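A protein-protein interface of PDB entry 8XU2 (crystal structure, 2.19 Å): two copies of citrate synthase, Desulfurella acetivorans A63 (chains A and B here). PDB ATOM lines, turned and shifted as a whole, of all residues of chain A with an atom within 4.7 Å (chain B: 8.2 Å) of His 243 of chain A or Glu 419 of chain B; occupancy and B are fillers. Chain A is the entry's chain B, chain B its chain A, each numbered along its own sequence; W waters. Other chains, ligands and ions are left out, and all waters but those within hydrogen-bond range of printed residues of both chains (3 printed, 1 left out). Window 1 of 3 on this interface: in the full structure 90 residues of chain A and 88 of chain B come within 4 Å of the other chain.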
ATOM      1  N   GLY A  42     -14.264 -22.776  12.743  1.00  0.00           N
ATOM      2  CA  GLY A  42     -12.884 -23.140  12.458  1.00  0.00           C
ATOM      3  C   GLY A  42     -12.664 -23.617  11.024  1.00  0.00           C
ATOM      4  O   GLY A  42     -11.915 -24.561  10.790  1.00  0.00           O
ATOM      5  N   MET A  43     -13.316 -22.938  10.072  1.00  0.00           N
ATOM      6  CA  MET A  43     -13.243 -23.245   8.651  1.00  0.00           C
ATOM      7  C   MET A  43     -13.566 -24.711   8.358  1.00  0.00           C
ATOM      8  O   MET A  43     -13.107 -25.253   7.362  1.00  0.00           O
ATOM      9  CB  MET A  43     -11.830 -22.966   8.129  1.00  0.00           C
ATOM     10  CG  MET A  43     -11.343 -21.536   8.355  1.00  0.00           C
ATOM     11  SD  MET A  43      -9.718 -21.353   7.626  1.00  0.00           S
ATOM     12  CE  MET A  43      -9.354 -19.642   7.991  1.00  0.00           C
ATOM     13  N   LEU A  49      -7.108 -25.132   0.933  1.00  0.00           N
ATOM     14  CA  LEU A  49      -5.673 -25.375   0.968  1.00  0.00           C
ATOM     15  C   LEU A  49      -5.303 -26.377  -0.120  1.00  0.00           C
ATOM     16  O   LEU A  49      -6.062 -27.304  -0.384  1.00  0.00           O
ATOM     17  CB  LEU A  49      -5.281 -25.936   2.339  1.00  0.00           C
ATOM     18  CG  LEU A  49      -5.305 -24.962   3.528  1.00  0.00           C
ATOM     19  CD1 LEU A  49      -5.074 -25.690   4.834  1.00  0.00           C
ATOM     20  CD2 LEU A  49      -4.295 -23.851   3.390  1.00  0.00           C
ATOM     21  N   SER A 237      -2.399 -30.679   4.711  1.00  0.00           N
ATOM     22  CA  SER A 237      -1.886 -29.394   5.161  1.00  0.00           C
ATOM     23  C   SER A 237      -2.869 -28.665   6.085  1.00  0.00           C
ATOM     24  O   SER A 237      -2.530 -27.600   6.601  1.00  0.00           O
ATOM     25  CB  SER A 237      -1.464 -28.547   3.983  1.00  0.00           C
ATOM     26  OG  SER A 237      -2.536 -28.117   3.179  1.00  0.00           O
ATOM     27  N   GLY A 238      -4.058 -29.247   6.302  1.00  0.00           N
ATOM     28  CA  GLY A 238      -5.139 -28.567   6.992  1.00  0.00           C
ATOM     29  C   GLY A 238      -5.165 -28.803   8.504  1.00  0.00           C
ATOM     30  O   GLY A 238      -5.850 -28.073   9.220  1.00  0.00           O
ATOM     31  N   ASN A 239      -4.416 -29.798   8.991  1.00  0.00           N
ATOM     32  CA  ASN A 239      -4.229 -29.983  10.420  1.00  0.00           C
ATOM     33  C   ASN A 239      -3.486 -28.777  11.012  1.00  0.00           C
ATOM     34  O   ASN A 239      -2.845 -28.025  10.288  1.00  0.00           O
ATOM     35  CB  ASN A 239      -3.575 -31.350  10.680  1.00  0.00           C
ATOM     36  CG  ASN A 239      -2.120 -31.412  10.299  1.00  0.00           C
ATOM     37  OD1 ASN A 239      -1.289 -30.912  11.052  1.00  0.00           O
ATOM     38  ND2 ASN A 239      -1.808 -32.056   9.179  1.00  0.00           N
ATOM     39  N   VAL A 240      -3.643 -28.539  12.315  1.00  0.00           N
ATOM     40  CA  VAL A 240      -3.211 -27.269  12.905  1.00  0.00           C
ATOM     41  C   VAL A 240      -1.696 -27.079  12.766  1.00  0.00           C
ATOM     42  O   VAL A 240      -1.242 -26.002  12.393  1.00  0.00           O
ATOM     43  CB  VAL A 240      -3.654 -27.139  14.377  1.00  0.00           C
ATOM     44  CG1 VAL A 240      -2.946 -25.988  15.101  1.00  0.00           C
ATOM     45  CG2 VAL A 240      -5.160 -26.996  14.499  1.00  0.00           C
ATOM     46  N   SER A 241      -0.913 -28.126  13.039  1.00  0.00           N
ATOM     47  CA  SER A 241       0.538 -27.991  13.012  1.00  0.00           C
ATOM     48  C   SER A 241       1.031 -27.750  11.581  1.00  0.00           C
ATOM     49  O   SER A 241       1.831 -26.842  11.328  1.00  0.00           O
ATOM     50  CB  SER A 241       1.211 -29.160  13.696  1.00  0.00           C
ATOM     51  OG  SER A 241       0.921 -30.411  13.105  1.00  0.00           O
ATOM     52  N   ALA A 242       0.539 -28.536  10.610  1.00  0.00           N
ATOM     53  CA  ALA A 242       0.985 -28.399   9.228  1.00  0.00           C
ATOM     54  C   ALA A 242       0.541 -27.059   8.644  1.00  0.00           C
ATOM     55  O   ALA A 242       1.254 -26.411   7.878  1.00  0.00           O
ATOM     56  CB  ALA A 242       0.475 -29.552   8.414  1.00  0.00           C
ATOM     57  N   HIS A 243      -0.683 -26.662   8.989  1.00  0.00           N
ATOM     58  CA  HIS A 243      -1.241 -25.412   8.510  1.00  0.00           C
ATOM     59  C   HIS A 243      -0.456 -24.236   9.095  1.00  0.00           C
ATOM     60  O   HIS A 243      -0.173 -23.257   8.408  1.00  0.00           O
ATOM     61  CB  HIS A 243      -2.720 -25.389   8.888  1.00  0.00           C
ATOM     62  CG  HIS A 243      -3.496 -24.182   8.467  1.00  0.00           C
ATOM     63  ND1 HIS A 243      -4.725 -23.859   9.003  1.00  0.00           N
ATOM     64  CD2 HIS A 243      -3.167 -23.205   7.586  1.00  0.00           C
ATOM     65  CE1 HIS A 243      -5.137 -22.724   8.440  1.00  0.00           C
ATOM     66  NE2 HIS A 243      -4.201 -22.305   7.554  1.00  0.00           N
ATOM     67  N   THR A 244      -0.095 -24.336  10.376  1.00  0.00           N
ATOM     68  CA  THR A 244       0.649 -23.275  11.035  1.00  0.00           C
ATOM     69  C   THR A 244       1.978 -23.066  10.321  1.00  0.00           C
ATOM     70  O   THR A 244       2.337 -21.933  10.003  1.00  0.00           O
ATOM     71  CB  THR A 244       0.818 -23.555  12.535  1.00  0.00           C
ATOM     72  OG1 THR A 244      -0.466 -23.569  13.177  1.00  0.00           O
ATOM     73  CG2 THR A 244       1.680 -22.510  13.212  1.00  0.00           C
ATOM     74  N   ALA A 245       2.701 -24.167  10.056  1.00  0.00           N
ATOM     75  CA  ALA A 245       3.955 -24.085   9.325  1.00  0.00           C
ATOM     76  C   ALA A 245       3.751 -23.410   7.976  1.00  0.00           C
ATOM     77  O   ALA A 245       4.509 -22.524   7.564  1.00  0.00           O
ATOM     78  CB  ALA A 245       4.546 -25.473   9.150  1.00  0.00           C
ATOM     79  N   HIS A 246       2.730 -23.884   7.252  1.00  0.00           N
ATOM     80  CA  HIS A 246       2.433 -23.401   5.915  1.00  0.00           C
ATOM     81  C   HIS A 246       2.122 -21.901   5.951  1.00  0.00           C
ATOM     82  O   HIS A 246       2.632 -21.119   5.143  1.00  0.00           O
ATOM     83  CB  HIS A 246       1.263 -24.224   5.362  1.00  0.00           C
ATOM     84  CG  HIS A 246       0.664 -23.682   4.102  1.00  0.00           C
ATOM     85  ND1 HIS A 246       1.261 -23.794   2.861  1.00  0.00           N
ATOM     86  CD2 HIS A 246      -0.492 -22.967   3.958  1.00  0.00           C
ATOM     87  CE1 HIS A 246       0.486 -23.165   1.974  1.00  0.00           C
ATOM     88  NE2 HIS A 246      -0.614 -22.685   2.623  1.00  0.00           N
ATOM     89  N   LEU A 247       1.290 -21.510   6.916  1.00  0.00           N
ATOM     90  CA  LEU A 247       0.879 -20.122   7.081  1.00  0.00           C
ATOM     91  C   LEU A 247       2.082 -19.216   7.348  1.00  0.00           C
ATOM     92  O   LEU A 247       2.280 -18.192   6.675  1.00  0.00           O
ATOM     93  CB  LEU A 247      -0.136 -20.088   8.222  1.00  0.00           C
ATOM     94  CG  LEU A 247      -0.551 -18.711   8.736  1.00  0.00           C
ATOM     95  CD1 LEU A 247      -1.078 -17.813   7.647  1.00  0.00           C
ATOM     96  CD2 LEU A 247      -1.601 -18.883   9.802  1.00  0.00           C
ATOM     97  N   GLU A 419      -0.763 -16.441   2.842  1.00  0.00           N
ATOM     98  CA  GLU A 419      -2.091 -16.829   3.270  1.00  0.00           C
ATOM     99  C   GLU A 419      -2.721 -15.670   4.044  1.00  0.00           C
ATOM    100  O   GLU A 419      -2.177 -15.227   5.070  1.00  0.00           O
ATOM    101  CB  GLU A 419      -2.047 -18.125   4.070  1.00  0.00           C
ATOM    102  CG  GLU A 419      -3.408 -18.544   4.598  1.00  0.00           C
ATOM    103  CD  GLU A 419      -3.453 -19.926   5.204  1.00  0.00           C
ATOM    104  OE1 GLU A 419      -2.897 -20.881   4.584  1.00  0.00           O
ATOM    105  OE2 GLU A 419      -4.058 -20.050   6.299  1.00  0.00           O
ATOM    106  N   MET B  43      -5.791 -18.408   0.231  1.00  0.00           N
ATOM    107  CA  MET B  43      -7.149 -18.110   0.666  1.00  0.00           C
ATOM    108  C   MET B  43      -7.528 -16.643   0.427  1.00  0.00           C
ATOM    109  O   MET B  43      -8.361 -16.117   1.151  1.00  0.00           O
ATOM    110  CB  MET B  43      -7.288 -18.383   2.164  1.00  0.00           C
ATOM    111  CG  MET B  43      -6.958 -19.765   2.626  1.00  0.00           C
ATOM    112  SD  MET B  43      -7.273 -19.797   4.426  1.00  0.00           S
ATOM    113  CE  MET B  43      -6.901 -21.514   4.802  1.00  0.00           C
ATOM    114  N   SER B  48     -13.659 -16.287   5.987  1.00  0.00           N
ATOM    115  CA  SER B  48     -13.607 -17.584   6.655  1.00  0.00           C
ATOM    116  C   SER B  48     -13.204 -17.471   8.129  1.00  0.00           C
ATOM    117  O   SER B  48     -13.004 -18.501   8.787  1.00  0.00           O
ATOM    118  CB  SER B  48     -12.695 -18.540   5.902  1.00  0.00           C
ATOM    119  OG  SER B  48     -11.526 -17.880   5.442  1.00  0.00           O
ATOM    120  N   LEU B  49     -13.125 -16.234   8.646  1.00  0.00           N
ATOM    121  CA  LEU B  49     -12.701 -15.958  10.017  1.00  0.00           C
ATOM    122  C   LEU B  49     -13.669 -14.963  10.647  1.00  0.00           C
ATOM    123  O   LEU B  49     -14.145 -14.073   9.957  1.00  0.00           O
ATOM    124  CB  LEU B  49     -11.282 -15.354  10.037  1.00  0.00           C
ATOM    125  CG  LEU B  49     -10.121 -16.281   9.672  1.00  0.00           C
ATOM    126  CD1 LEU B  49      -8.840 -15.483   9.524  1.00  0.00           C
ATOM    127  CD2 LEU B  49      -9.942 -17.386  10.691  1.00  0.00           C
ATOM    128  N   VAL B  50     -13.860 -15.079  11.967  1.00  0.00           N
ATOM    129  CA  VAL B  50     -14.733 -14.202  12.717  1.00  0.00           C
ATOM    130  C   VAL B  50     -13.958 -13.614  13.891  1.00  0.00           C
ATOM    131  O   VAL B  50     -13.447 -14.350  14.731  1.00  0.00           O
ATOM    132  CB  VAL B  50     -15.989 -14.937  13.233  1.00  0.00           C
ATOM    133  CG1 VAL B  50     -16.979 -13.961  13.845  1.00  0.00           C
ATOM    134  CG2 VAL B  50     -16.647 -15.771  12.147  1.00  0.00           C
ATOM    135  N   SER B 237      -8.310 -10.465  12.083  1.00  0.00           N
ATOM    136  CA  SER B 237      -7.728 -11.735  12.476  1.00  0.00           C
ATOM    137  C   SER B 237      -7.095 -12.462  11.291  1.00  0.00           C
ATOM    138  O   SER B 237      -6.490 -13.514  11.494  1.00  0.00           O
ATOM    139  CB  SER B 237      -8.749 -12.599  13.196  1.00  0.00           C
ATOM    140  OG  SER B 237      -9.812 -13.018  12.352  1.00  0.00           O
ATOM    141  N   ALA B 242      -1.841 -12.488  13.384  1.00  0.00           N
ATOM    142  CA  ALA B 242      -3.042 -12.642  14.188  1.00  0.00           C
ATOM    143  C   ALA B 242      -3.693 -13.993  13.914  1.00  0.00           C
ATOM    144  O   ALA B 242      -4.231 -14.647  14.814  1.00  0.00           O
ATOM    145  CB  ALA B 242      -3.985 -11.496  13.916  1.00  0.00           C
ATOM    146  N   HIS B 243      -3.685 -14.392  12.653  1.00  0.00           N
ATOM    147  CA  HIS B 243      -4.264 -15.660  12.247  1.00  0.00           C
ATOM    148  C   HIS B 243      -3.475 -16.814  12.854  1.00  0.00           C
ATOM    149  O   HIS B 243      -4.041 -17.801  13.318  1.00  0.00           O
ATOM    150  CB  HIS B 243      -4.279 -15.694  10.712  1.00  0.00           C
ATOM    151  CG  HIS B 243      -4.901 -16.909  10.098  1.00  0.00           C
ATOM    152  ND1 HIS B 243      -4.759 -17.231   8.771  1.00  0.00           N
ATOM    153  CD2 HIS B 243      -5.649 -17.892  10.674  1.00  0.00           C
ATOM    154  CE1 HIS B 243      -5.413 -18.370   8.549  1.00  0.00           C
ATOM    155  NE2 HIS B 243      -5.955 -18.806   9.710  1.00  0.00           N
ATOM    156  N   THR B 244      -2.145 -16.693  12.855  1.00  0.00           N
ATOM    157  CA  THR B 244      -1.296 -17.743  13.411  1.00  0.00           C
ATOM    158  C   THR B 244      -1.617 -17.930  14.882  1.00  0.00           C
ATOM    159  O   THR B 244      -1.798 -19.050  15.343  1.00  0.00           O
ATOM    160  CB  THR B 244       0.196 -17.450  13.167  1.00  0.00           C
ATOM    161  OG1 THR B 244       0.450 -17.432  11.750  1.00  0.00           O
ATOM    162  CG2 THR B 244       1.093 -18.469  13.834  1.00  0.00           C
ATOM    163  N   ALA B 245      -1.697 -16.819  15.640  1.00  0.00           N
ATOM    164  CA  ALA B 245      -2.054 -16.903  17.055  1.00  0.00           C
ATOM    165  C   ALA B 245      -3.408 -17.604  17.215  1.00  0.00           C
ATOM    166  O   ALA B 245      -3.579 -18.491  18.054  1.00  0.00           O
ATOM    167  CB  ALA B 245      -2.097 -15.516  17.655  1.00  0.00           C
ATOM    168  N   HIS B 246      -4.385 -17.159  16.413  1.00  0.00           N
ATOM    169  CA  HIS B 246      -5.746 -17.670  16.488  1.00  0.00           C
ATOM    170  C   HIS B 246      -5.760 -19.170  16.202  1.00  0.00           C
ATOM    171  O   HIS B 246      -6.381 -19.961  16.919  1.00  0.00           O
ATOM    172  CB  HIS B 246      -6.615 -16.878  15.502  1.00  0.00           C
ATOM    173  CG  HIS B 246      -7.979 -17.454  15.280  1.00  0.00           C
ATOM    174  ND1 HIS B 246      -9.018 -17.374  16.179  1.00  0.00           N
ATOM    175  CD2 HIS B 246      -8.426 -18.176  14.227  1.00  0.00           C
ATOM    176  CE1 HIS B 246     -10.071 -18.017  15.680  1.00  0.00           C
ATOM    177  NE2 HIS B 246      -9.744 -18.477  14.458  1.00  0.00           N
ATOM    178  N   LEU B 247      -5.052 -19.554  15.135  1.00  0.00           N
ATOM    179  CA  LEU B 247      -4.964 -20.946  14.716  1.00  0.00           C
ATOM    180  C   LEU B 247      -4.369 -21.824  15.811  1.00  0.00           C
ATOM    181  O   LEU B 247      -4.931 -22.862  16.192  1.00  0.00           O
ATOM    182  CB  LEU B 247      -4.129 -20.964  13.434  1.00  0.00           C
ATOM    183  CG  LEU B 247      -3.690 -22.325  12.907  1.00  0.00           C
ATOM    184  CD1 LEU B 247      -4.865 -23.254  12.686  1.00  0.00           C
ATOM    185  CD2 LEU B 247      -2.919 -22.119  11.633  1.00  0.00           C
ATOM    186  N   VAL B 248      -3.221 -21.398  16.337  1.00  0.00           N
ATOM    187  CA  VAL B 248      -2.523 -22.183  17.350  1.00  0.00           C
ATOM    188  C   VAL B 248      -3.388 -22.305  18.597  1.00  0.00           C
ATOM    189  O   VAL B 248      -3.574 -23.406  19.107  1.00  0.00           O
ATOM    190  CB  VAL B 248      -1.123 -21.583  17.607  1.00  0.00           C
ATOM    191  CG1 VAL B 248      -0.484 -22.108  18.874  1.00  0.00           C
ATOM    192  CG2 VAL B 248      -0.230 -21.824  16.390  1.00  0.00           C
ATOM    193  N   ALA B 249      -3.947 -21.176  19.074  1.00  0.00           N
ATOM    194  CA  ALA B 249      -4.819 -21.163  20.241  1.00  0.00           C
ATOM    195  C   ALA B 249      -6.098 -21.999  20.055  1.00  0.00           C
ATOM    196  O   ALA B 249      -6.656 -22.498  21.047  1.00  0.00           O
ATOM    197  CB  ALA B 249      -5.169 -19.745  20.606  1.00  0.00           C
ATOM    198  N   SER B 250      -6.551 -22.152  18.801  1.00  0.00           N
ATOM    199  CA  SER B 250      -7.741 -22.936  18.484  1.00  0.00           C
ATOM    200  C   SER B 250      -7.570 -24.409  18.880  1.00  0.00           C
ATOM    201  O   SER B 250      -8.582 -25.094  19.151  1.00  0.00           O
ATOM    202  CB  SER B 250      -8.137 -22.790  17.025  1.00  0.00           C
ATOM    203  OG  SER B 250      -7.360 -23.639  16.181  1.00  0.00           O
ATOM    204  N   ALA B 251      -6.303 -24.882  18.971  1.00  0.00           N
ATOM    205  CA  ALA B 251      -6.028 -26.228  19.461  1.00  0.00           C
ATOM    206  C   ALA B 251      -5.900 -26.253  20.989  1.00  0.00           C
ATOM    207  O   ALA B 251      -5.541 -27.279  21.551  1.00  0.00           O
ATOM    208  CB  ALA B 251      -4.819 -26.801  18.787  1.00  0.00           C
ATOM    209  N   LEU B 252      -6.209 -25.118  21.638  1.00  0.00           N
ATOM    210  CA  LEU B 252      -6.174 -24.905  23.082  1.00  0.00           C
ATOM    211  C   LEU B 252      -4.738 -24.808  23.614  1.00  0.00           C
ATOM    212  O   LEU B 252      -4.513 -24.958  24.821  1.00  0.00           O
ATOM    213  CB  LEU B 252      -7.005 -25.972  23.815  1.00  0.00           C
ATOM    214  CG  LEU B 252      -8.507 -25.988  23.501  1.00  0.00           C
ATOM    215  CD1 LEU B 252      -9.221 -26.950  24.448  1.00  0.00           C
ATOM    216  CD2 LEU B 252      -9.112 -24.584  23.610  1.00  0.00           C
ATOM    217  N   ASP B 411     -11.873 -15.726  21.668  1.00  0.00           N
ATOM    218  CA  ASP B 411     -11.976 -17.032  21.029  1.00  0.00           C
ATOM    219  C   ASP B 411     -12.367 -18.068  22.074  1.00  0.00           C
ATOM    220  O   ASP B 411     -13.210 -18.912  21.811  1.00  0.00           O
ATOM    221  CB  ASP B 411     -10.680 -17.481  20.346  1.00  0.00           C
ATOM    222  CG  ASP B 411     -10.293 -16.700  19.101  1.00  0.00           C
ATOM    223  OD1 ASP B 411     -11.164 -15.994  18.532  1.00  0.00           O
ATOM    224  OD2 ASP B 411      -9.105 -16.791  18.695  1.00  0.00           O
ATOM    225  N   ARG B 412     -11.750 -18.009  23.259  1.00  0.00           N
ATOM    226  CA  ARG B 412     -12.063 -18.963  24.311  1.00  0.00           C
ATOM    227  C   ARG B 412     -13.418 -18.649  24.953  1.00  0.00           C
ATOM    228  O   ARG B 412     -14.117 -19.577  25.366  1.00  0.00           O
ATOM    229  CB  ARG B 412     -10.966 -19.005  25.380  1.00  0.00           C
ATOM    230  CG  ARG B 412      -9.619 -19.501  24.864  1.00  0.00           C
ATOM    231  CD  ARG B 412      -9.596 -20.958  24.420  1.00  0.00           C
ATOM    232  NE  ARG B 412     -10.307 -21.229  23.176  1.00  0.00           N
ATOM    233  CZ  ARG B 412      -9.918 -20.861  21.967  1.00  0.00           C
ATOM    234  NH1 ARG B 412     -10.698 -21.135  20.935  1.00  0.00           N
ATOM    235  NH2 ARG B 412      -8.753 -20.252  21.787  1.00  0.00           N
ATOM    236  N   TYR B 416     -14.794 -20.898  20.186  1.00  0.00           N
ATOM    237  CA  TYR B 416     -14.480 -21.155  18.790  1.00  0.00           C
ATOM    238  C   TYR B 416     -13.685 -22.460  18.646  1.00  0.00           C
ATOM    239  O   TYR B 416     -12.787 -22.769  19.426  1.00  0.00           O
ATOM    240  CB  TYR B 416     -13.760 -19.954  18.169  1.00  0.00           C
ATOM    241  CG  TYR B 416     -14.617 -18.737  17.900  1.00  0.00           C
ATOM    242  CD1 TYR B 416     -16.004 -18.785  17.913  1.00  0.00           C
ATOM    243  CD2 TYR B 416     -14.027 -17.515  17.636  1.00  0.00           C
ATOM    244  CE1 TYR B 416     -16.766 -17.663  17.652  1.00  0.00           C
ATOM    245  CE2 TYR B 416     -14.775 -16.371  17.390  1.00  0.00           C
ATOM    246  CZ  TYR B 416     -16.157 -16.449  17.384  1.00  0.00           C
ATOM    247  OH  TYR B 416     -16.921 -15.332  17.121  1.00  0.00           O
ATOM    248  N   ALA B 417     -14.061 -23.241  17.639  1.00  0.00           N
ATOM    249  CA  ALA B 417     -13.593 -24.609  17.482  1.00  0.00           C
ATOM    250  C   ALA B 417     -12.212 -24.606  16.839  1.00  0.00           C
ATOM    251  O   ALA B 417     -11.788 -23.599  16.260  1.00  0.00           O
ATOM    252  CB  ALA B 417     -14.577 -25.394  16.631  1.00  0.00           C
ATOM    253  N   ILE B 418     -11.535 -25.762  16.919  1.00  0.00           N
ATOM    254  CA  ILE B 418     -10.237 -25.937  16.293  1.00  0.00           C
ATOM    255  C   ILE B 418     -10.349 -25.554  14.822  1.00  0.00           C
ATOM    256  O   ILE B 418     -11.294 -25.949  14.142  1.00  0.00           O
ATOM    257  CB  ILE B 418      -9.701 -27.370  16.521  1.00  0.00           C
ATOM    258  CG1 ILE B 418      -8.229 -27.481  16.105  1.00  0.00           C
ATOM    259  CG2 ILE B 418     -10.563 -28.430  15.829  1.00  0.00           C
ATOM    260  CD1 ILE B 418      -7.566 -28.801  16.397  1.00  0.00           C
ATOM    261  N   GLU B 419      -9.388 -24.747  14.341  1.00  0.00           N
ATOM    262  CA  GLU B 419      -9.337 -24.376  12.940  1.00  0.00           C
ATOM    263  C   GLU B 419      -8.688 -25.508  12.145  1.00  0.00           C
ATOM    264  O   GLU B 419      -7.544 -25.898  12.401  1.00  0.00           O
ATOM    265  CB  GLU B 419      -8.596 -23.050  12.768  1.00  0.00           C
ATOM    266  CG  GLU B 419      -8.477 -22.620  11.328  1.00  0.00           C
ATOM    267  CD  GLU B 419      -7.934 -21.228  11.110  1.00  0.00           C
ATOM    268  OE1 GLU B 419      -8.362 -20.312  11.819  1.00  0.00           O
ATOM    269  OE2 GLU B 419      -7.098 -21.066  10.225  1.00  0.00           O
ATOM    270  N   ARG B 420      -9.453 -26.053  11.194  1.00  0.00           N
ATOM    271  CA  ARG B 420      -9.077 -27.263  10.485  1.00  0.00           C
ATOM    272  C   ARG B 420      -9.808 -27.282   9.144  1.00  0.00           C
ATOM    273  O   ARG B 420     -10.815 -27.967   8.984  1.00  0.00           O
ATOM    274  CB  ARG B 420      -9.412 -28.496  11.339  1.00  0.00           C
ATOM    275  CG  ARG B 420      -8.484 -29.685  11.098  1.00  0.00           C
ATOM    276  CD  ARG B 420      -8.375 -30.114   9.645  1.00  0.00           C
ATOM    277  NE  ARG B 420      -7.681 -31.388   9.458  1.00  0.00           N
ATOM    278  CZ  ARG B 420      -7.100 -31.770   8.311  1.00  0.00           C
ATOM    279  NH1 ARG B 420      -7.271 -31.063   7.204  1.00  0.00           N
ATOM    280  NH2 ARG B 420      -6.317 -32.844   8.275  1.00  0.00           N
ATOM    281  N   PRO B 421      -9.348 -26.495   8.150  1.00  0.00           N
ATOM    282  CA  PRO B 421      -9.892 -26.582   6.798  1.00  0.00           C
ATOM    283  C   PRO B 421      -9.444 -27.886   6.129  1.00  0.00           C
ATOM    284  O   PRO B 421      -8.678 -28.659   6.708  1.00  0.00           O
ATOM    285  CB  PRO B 421      -9.306 -25.337   6.115  1.00  0.00           C
ATOM    286  CG  PRO B 421      -7.997 -25.056   6.865  1.00  0.00           C
ATOM    287  CD  PRO B 421      -8.229 -25.540   8.277  1.00  0.00           C
ATOM    288  N   LYS B 422      -9.898 -28.087   4.884  1.00  0.00           N
ATOM    289  CA  LYS B 422      -9.631 -29.281   4.106  1.00  0.00           C
ATOM    290  C   LYS B 422      -8.654 -28.935   2.993  1.00  0.00           C
ATOM    291  O   LYS B 422      -8.788 -27.883   2.382  1.00  0.00           O
ATOM    292  CB  LYS B 422     -10.949 -29.859   3.562  1.00  0.00           C
ATOM    293  CG  LYS B 422     -10.838 -31.216   2.865  1.00  0.00           C
ATOM    294  CD  LYS B 422     -10.577 -32.368   3.847  1.00  0.00           C
ATOM    295  CE  LYS B 422     -10.314 -33.692   3.173  1.00  0.00           C
ATOM    296  NZ  LYS B 422      -9.129 -33.661   2.284  1.00  0.00           N
ATOM    297  N   SER B 423      -7.661 -29.817   2.767  1.00  0.00           N
ATOM    298  CA  SER B 423      -6.733 -29.694   1.651  1.00  0.00           C
ATOM    299  C   SER B 423      -7.290 -30.412   0.424  1.00  0.00           C
ATOM    300  O   SER B 423      -8.013 -31.388   0.543  1.00  0.00           O
ATOM    301  CB  SER B 423      -5.335 -30.253   1.968  1.00  0.00           C
ATOM    302  OG  SER B 423      -4.884 -29.806   3.233  1.00  0.00           O
HETATM  303  O   HOH W   1      -3.355 -15.257   7.479  1.00  0.00           O
HETATM  304  O   HOH W   2     -12.852 -19.794  10.919  1.00  0.00           O
HETATM  305  O   HOH W   3     -10.733 -20.817   4.417  1.00  0.00           O
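Glu 419 of chain B touches just these residues of chain A: Gly 42, Met 43, Val 240 and His 243.
No residue of chain B comes within 4 Å of Ala 242 of chain A.
Printed residues of chain A within 4 Å of His 243 of chain B: Met 43, Leu 247 and Glu 419.
Ala 242 of chain B touches none of the printed residues of chain A.
The nearest residue of chain B that does not touch His 243 of chain A is His 243 of chain B (4.2 Å).
The nearest residue of chain A that does not touch Glu 419 of chain B is Gly 238 of chain A (4.2 Å).
Water W3 lies within hydrogen-bond range of OG of Ser 48 of chain B (3.2 Å), SD of Met 43 of chain A (3.4 Å) and SD of Met 43 of chain B (3.6 Å).
Met 43 of chain A touches its own counterpart, Met 43 of chain B.
Of the 34 pairs that touch across the chains among the printed residues, 14 have their exchanged pair printed and touching as well.
The side-chain carboxylate (OE2) of Glu 419 of chain A sits close to the side-chain sulfur (SD) of Met 43 of chain B (3.7 Å).
SD of Met 43 of chain A lies close to OE2 of Glu 419 of chain B (3.7 Å).
The side-chain hydroxyl (OG) of Ser 423 of chain B is in hydrogen-bond range of the backbone NH (N) of Gly 238 of chain A.
The side-chain hydroxyl of Ser 423 of chain B sits at hydrogen-bond distance from the side-chain hydroxyl of Ser 237 of chain A (2.9 Å).
The backbone NH of Arg 420 of chain B sits at hydrogen-bond distance from the backbone carbonyl oxygen of Gly 42 of chain A (2.9 Å).
O of Ser 237 of chain A is in hydrogen-bond range of N of His 243 of chain A (3.2 Å).
OD1 of Asn 239 of chain A sits at hydrogen-bond distance from N of Ala 242 of chain A, at 3.0 Å.
Of the 26 printed residues of chain B, 14 touch a printed residue of chain A.
Of the 15 printed residues of chain A, 11 touch a printed residue of chain B.
Along chain A the printed residues that touch a printed residue of chain B span positions 42 to 419.
Among the printed residues, no Asp or Glu carboxylate lies within 4 Å of a Lys or Arg side-chain nitrogen of the other chain.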
